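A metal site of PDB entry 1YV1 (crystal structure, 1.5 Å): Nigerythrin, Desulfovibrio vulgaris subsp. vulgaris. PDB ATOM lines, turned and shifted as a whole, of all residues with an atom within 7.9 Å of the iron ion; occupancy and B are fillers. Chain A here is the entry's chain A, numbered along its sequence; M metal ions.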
ATOM      1  N   ARG A 144     -21.331  14.031 -14.709  1.00  0.00           N
ATOM      2  CA  ARG A 144     -20.648  14.874 -15.671  1.00  0.00           C
ATOM      3  C   ARG A 144     -21.620  15.645 -16.563  1.00  0.00           C
ATOM      4  O   ARG A 144     -21.441  16.844 -16.791  1.00  0.00           O
ATOM      5  CB  ARG A 144     -19.698  14.013 -16.520  1.00  0.00           C
ATOM      6  CG  ARG A 144     -18.453  13.559 -15.772  1.00  0.00           C
ATOM      7  CD  ARG A 144     -17.573  14.752 -15.431  1.00  0.00           C
ATOM      8  NE  ARG A 144     -16.462  14.437 -14.528  1.00  0.00           N
ATOM      9  CZ  ARG A 144     -15.389  13.726 -14.858  1.00  0.00           C
ATOM     10  NH1 ARG A 144     -15.247  13.234 -16.083  1.00  0.00           N
ATOM     11  NH2 ARG A 144     -14.423  13.529 -13.957  1.00  0.00           N
ATOM     12  N   ALA A 148     -22.322  19.818 -16.637  1.00  0.00           N
ATOM     13  CA  ALA A 148     -22.164  20.553 -17.879  1.00  0.00           C
ATOM     14  C   ALA A 148     -23.430  21.330 -18.251  1.00  0.00           C
ATOM     15  O   ALA A 148     -23.346  22.458 -18.735  1.00  0.00           O
ATOM     16  CB  ALA A 148     -21.796  19.597 -19.010  1.00  0.00           C
ATOM     17  N   LEU A 173     -14.678  24.008 -25.954  1.00  0.00           N
ATOM     18  CA  LEU A 173     -15.399  22.829 -25.508  1.00  0.00           C
ATOM     19  C   LEU A 173     -14.497  21.722 -24.983  1.00  0.00           C
ATOM     20  O   LEU A 173     -13.556  21.314 -25.664  1.00  0.00           O
ATOM     21  CB  LEU A 173     -16.241  22.287 -26.667  1.00  0.00           C
ATOM     22  CG  LEU A 173     -17.008  20.978 -26.427  1.00  0.00           C
ATOM     23  CD1 LEU A 173     -18.152  21.234 -25.461  1.00  0.00           C
ATOM     24  CD2 LEU A 173     -17.538  20.458 -27.755  1.00  0.00           C
ATOM     25  N   CYS A 174     -14.791  21.236 -23.781  1.00  0.00           N
ATOM     26  CA  CYS A 174     -14.017  20.149 -23.199  1.00  0.00           C
ATOM     27  C   CYS A 174     -14.499  18.849 -23.846  1.00  0.00           C
ATOM     28  O   CYS A 174     -15.689  18.542 -23.811  1.00  0.00           O
ATOM     29  CB  CYS A 174     -14.238  20.070 -21.690  1.00  0.00           C
ATOM     30  SG  CYS A 174     -13.438  18.623 -20.943  1.00  0.00           S
ATOM     31  N   PRO A 175     -13.585  18.071 -24.449  1.00  0.00           N
ATOM     32  CA  PRO A 175     -13.942  16.814 -25.119  1.00  0.00           C
ATOM     33  C   PRO A 175     -14.401  15.695 -24.195  1.00  0.00           C
ATOM     34  O   PRO A 175     -15.010  14.722 -24.640  1.00  0.00           O
ATOM     35  CB  PRO A 175     -12.672  16.448 -25.855  1.00  0.00           C
ATOM     36  CG  PRO A 175     -11.607  16.947 -24.926  1.00  0.00           C
ATOM     37  CD  PRO A 175     -12.135  18.312 -24.532  1.00  0.00           C
ATOM     38  N   ILE A 176     -14.112  15.845 -22.906  1.00  0.00           N
ATOM     39  CA  ILE A 176     -14.457  14.816 -21.934  1.00  0.00           C
ATOM     40  C   ILE A 176     -15.826  14.957 -21.265  1.00  0.00           C
ATOM     41  O   ILE A 176     -16.539  13.970 -21.101  1.00  0.00           O
ATOM     42  CB  ILE A 176     -13.370  14.745 -20.833  1.00  0.00           C
ATOM     43  CG1 ILE A 176     -12.008  14.431 -21.469  1.00  0.00           C
ATOM     44  CG2 ILE A 176     -13.714  13.675 -19.812  1.00  0.00           C
ATOM     45  CD1 ILE A 176     -11.977  13.151 -22.264  1.00  0.00           C
ATOM     46  N   CYS A 177     -16.218  16.179 -20.899  1.00  0.00           N
ATOM     47  CA  CYS A 177     -17.489  16.373 -20.216  1.00  0.00           C
ATOM     48  C   CYS A 177     -18.465  17.348 -20.850  1.00  0.00           C
ATOM     49  O   CYS A 177     -19.611  17.445 -20.412  1.00  0.00           O
ATOM     50  CB  CYS A 177     -17.215  16.811 -18.777  1.00  0.00           C
ATOM     51  SG  CYS A 177     -16.531  18.468 -18.649  1.00  0.00           S
ATOM     52  N   GLY A 178     -18.028  18.084 -21.860  1.00  0.00           N
ATOM     53  CA  GLY A 178     -18.939  19.025 -22.489  1.00  0.00           C
ATOM     54  C   GLY A 178     -18.949  20.408 -21.882  1.00  0.00           C
ATOM     55  O   GLY A 178     -19.799  21.233 -22.215  1.00  0.00           O
ATOM     56  N   TYR A 179     -18.028  20.681 -20.976  1.00  0.00           N
ATOM     57  CA  TYR A 179     -17.928  21.991 -20.368  1.00  0.00           C
ATOM     58  C   TYR A 179     -17.591  22.981 -21.483  1.00  0.00           C
ATOM     59  O   TYR A 179     -16.868  22.647 -22.413  1.00  0.00           O
ATOM     60  CB  TYR A 179     -16.813  22.008 -19.321  1.00  0.00           C
ATOM     61  CG  TYR A 179     -16.411  23.394 -18.852  1.00  0.00           C
ATOM     62  CD1 TYR A 179     -17.220  24.119 -17.986  1.00  0.00           C
ATOM     63  CD2 TYR A 179     -15.224  23.984 -19.294  1.00  0.00           C
ATOM     64  CE1 TYR A 179     -16.864  25.400 -17.553  1.00  0.00           C
ATOM     65  CE2 TYR A 179     -14.842  25.256 -18.876  1.00  0.00           C
ATOM     66  CZ  TYR A 179     -15.676  25.956 -17.997  1.00  0.00           C
ATOM     67  OH  TYR A 179     -15.309  27.203 -17.555  1.00  0.00           O
ATOM     68  N   ILE A 180     -18.121  24.198 -21.378  1.00  0.00           N
ATOM     69  CA  ILE A 180     -17.840  25.231 -22.367  1.00  0.00           C
ATOM     70  C   ILE A 180     -17.368  26.490 -21.681  1.00  0.00           C
ATOM     71  O   ILE A 180     -17.966  26.944 -20.703  1.00  0.00           O
ATOM     72  CB  ILE A 180     -19.098  25.590 -23.203  1.00  0.00           C
ATOM     73  CG1 ILE A 180     -19.512  24.379 -24.045  1.00  0.00           C
ATOM     74  CG2 ILE A 180     -18.822  26.800 -24.094  1.00  0.00           C
ATOM     75  CD1 ILE A 180     -20.824  24.562 -24.773  1.00  0.00           C
ATOM     76  N   LYS A 188      -7.793  25.017 -17.235  1.00  0.00           N
ATOM     77  CA  LYS A 188      -8.333  23.670 -17.320  1.00  0.00           C
ATOM     78  C   LYS A 188      -9.834  23.636 -17.061  1.00  0.00           C
ATOM     79  O   LYS A 188     -10.425  24.617 -16.614  1.00  0.00           O
ATOM     80  CB  LYS A 188      -7.628  22.757 -16.317  1.00  0.00           C
ATOM     81  CG  LYS A 188      -7.886  23.105 -14.862  1.00  0.00           C
ATOM     82  CD  LYS A 188      -7.176  22.130 -13.926  1.00  0.00           C
ATOM     83  CE  LYS A 188      -7.434  22.475 -12.461  1.00  0.00           C
ATOM     84  NZ  LYS A 188      -6.691  21.561 -11.536  1.00  0.00           N
ATOM     85  N   CYS A 189     -10.435  22.485 -17.358  1.00  0.00           N
ATOM     86  CA  CYS A 189     -11.865  22.288 -17.164  1.00  0.00           C
ATOM     87  C   CYS A 189     -12.166  22.195 -15.666  1.00  0.00           C
ATOM     88  O   CYS A 189     -11.556  21.402 -14.945  1.00  0.00           O
ATOM     89  CB  CYS A 189     -12.296  21.003 -17.861  1.00  0.00           C
ATOM     90  SG  CYS A 189     -14.047  20.624 -17.652  1.00  0.00           S
ATOM     91  N   PRO A 190     -13.124  22.998 -15.169  1.00  0.00           N
ATOM     92  CA  PRO A 190     -13.471  22.962 -13.745  1.00  0.00           C
ATOM     93  C   PRO A 190     -14.284  21.726 -13.358  1.00  0.00           C
ATOM     94  O   PRO A 190     -14.437  21.423 -12.170  1.00  0.00           O
ATOM     95  CB  PRO A 190     -14.255  24.255 -13.556  1.00  0.00           C
ATOM     96  CG  PRO A 190     -14.967  24.388 -14.868  1.00  0.00           C
ATOM     97  CD  PRO A 190     -13.870  24.060 -15.869  1.00  0.00           C
ATOM     98  N   ILE A 191     -14.804  21.016 -14.361  1.00  0.00           N
ATOM     99  CA  ILE A 191     -15.593  19.826 -14.098  1.00  0.00           C
ATOM    100  C   ILE A 191     -14.748  18.553 -14.047  1.00  0.00           C
ATOM    101  O   ILE A 191     -14.933  17.725 -13.148  1.00  0.00           O
ATOM    102  CB  ILE A 191     -16.704  19.650 -15.171  1.00  0.00           C
ATOM    103  CG1 ILE A 191     -17.726  20.779 -15.020  1.00  0.00           C
ATOM    104  CG2 ILE A 191     -17.381  18.285 -15.021  1.00  0.00           C
ATOM    105  CD1 ILE A 191     -18.813  20.775 -16.074  1.00  0.00           C
ATOM    106  N   CYS A 192     -13.817  18.390 -14.989  1.00  0.00           N
ATOM    107  CA  CYS A 192     -12.981  17.190 -15.018  1.00  0.00           C
ATOM    108  C   CYS A 192     -11.477  17.437 -15.006  1.00  0.00           C
ATOM    109  O   CYS A 192     -10.684  16.497 -15.075  1.00  0.00           O
ATOM    110  CB  CYS A 192     -13.338  16.328 -16.236  1.00  0.00           C
ATOM    111  SG  CYS A 192     -12.840  17.040 -17.824  1.00  0.00           S
ATOM    112  N   PHE A 193     -11.082  18.711 -14.930  1.00  0.00           N
ATOM    113  CA  PHE A 193      -9.676  19.117 -14.897  1.00  0.00           C
ATOM    114  C   PHE A 193      -8.881  18.929 -16.193  1.00  0.00           C
ATOM    115  O   PHE A 193      -7.659  19.046 -16.204  1.00  0.00           O
ATOM    116  CB  PHE A 193      -8.951  18.391 -13.741  1.00  0.00           C
ATOM    117  CG  PHE A 193      -9.301  18.935 -12.379  1.00  0.00           C
ATOM    118  CD1 PHE A 193     -10.317  19.855 -12.210  1.00  0.00           C
ATOM    119  CD2 PHE A 193      -8.593  18.512 -11.260  1.00  0.00           C
ATOM    120  CE1 PHE A 193     -10.644  20.352 -10.941  1.00  0.00           C
ATOM    121  CE2 PHE A 193      -8.894  18.995  -9.988  1.00  0.00           C
ATOM    122  CZ  PHE A 193      -9.920  19.915  -9.828  1.00  0.00           C
ATOM    123  N   ARG A 194      -9.584  18.647 -17.274  1.00  0.00           N
ATOM    124  CA  ARG A 194      -8.944  18.478 -18.566  1.00  0.00           C
ATOM    125  C   ARG A 194      -8.191  19.763 -18.932  1.00  0.00           C
ATOM    126  O   ARG A 194      -8.765  20.849 -18.916  1.00  0.00           O
ATOM    127  CB  ARG A 194      -9.995  18.186 -19.633  1.00  0.00           C
ATOM    128  CG  ARG A 194      -9.446  17.771 -20.989  1.00  0.00           C
ATOM    129  CD  ARG A 194      -8.840  16.388 -20.913  1.00  0.00           C
ATOM    130  NE  ARG A 194      -8.618  15.806 -22.240  1.00  0.00           N
ATOM    131  CZ  ARG A 194      -8.306  14.538 -22.447  1.00  0.00           C
ATOM    132  NH1 ARG A 194      -8.176  13.718 -21.412  1.00  0.00           N
ATOM    133  NH2 ARG A 194      -8.134  14.083 -23.681  1.00  0.00           N
ATOM    134  N   PRO A 195      -6.891  19.655 -19.254  1.00  0.00           N
ATOM    135  CA  PRO A 195      -6.126  20.843 -19.624  1.00  0.00           C
ATOM    136  C   PRO A 195      -6.693  21.530 -20.877  1.00  0.00           C
ATOM    137  O   PRO A 195      -7.234  20.855 -21.760  1.00  0.00           O
ATOM    138  CB  PRO A 195      -4.724  20.296 -19.857  1.00  0.00           C
ATOM    139  CG  PRO A 195      -4.657  19.174 -18.866  1.00  0.00           C
ATOM    140  CD  PRO A 195      -6.005  18.505 -19.043  1.00  0.00           C
ATOM    141  N   PHE A 199      -8.853  21.096 -25.641  1.00  0.00           N
ATOM    142  CA  PHE A 199     -10.199  21.617 -25.900  1.00  0.00           C
ATOM    143  C   PHE A 199     -10.290  21.926 -27.393  1.00  0.00           C
ATOM    144  O   PHE A 199      -9.273  21.983 -28.088  1.00  0.00           O
ATOM    145  CB  PHE A 199     -10.428  22.927 -25.137  1.00  0.00           C
ATOM    146  CG  PHE A 199     -10.927  22.752 -23.734  1.00  0.00           C
ATOM    147  CD1 PHE A 199     -10.232  21.979 -22.808  1.00  0.00           C
ATOM    148  CD2 PHE A 199     -12.077  23.421 -23.309  1.00  0.00           C
ATOM    149  CE1 PHE A 199     -10.674  21.871 -21.490  1.00  0.00           C
ATOM    150  CE2 PHE A 199     -12.521  23.324 -21.998  1.00  0.00           C
ATOM    151  CZ  PHE A 199     -11.815  22.549 -21.083  1.00  0.00           C
HETATM  152 FE    FE M   1     -14.243  18.587 -18.758  1.00  0.00          FE
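The backbone NH of Arg 194 sits close to the side-chain sulfur of Cys 192 (3.7 Å). The side-chain sulfur (SG) of Cys 177 lies close to the backbone NH (N) of Tyr 179 (3.5 Å). The backbone carbonyl oxygen (O) of Arg 194 sits at hydrogen-bond distance from the backbone NH (N) of Cys 189. N of Ile 191 sits close to SG of Cys 189, 3.4 Å away. The backbone NH of Cys 174 is in hydrogen-bond range of the backbone carbonyl oxygen of Tyr 179 (2.9 Å). The backbone NH of Ile 176 lies close to the side-chain sulfur of Cys 174 (3.5 Å).
The nearest printed residue that does not touch the iron ion is Tyr 179 (4.3 Å).
The iron ion is bound by SG of Cys 192 (2.3 Å). The iron ion is bound by the side-chain sulfur (SG) of Cys 177. The iron ion is bound by SG of Cys 189 (2.3 Å). The iron ion is bound by SG of Cys 174 (2.3 Å). The iron ion has four donor atoms within binding distance.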
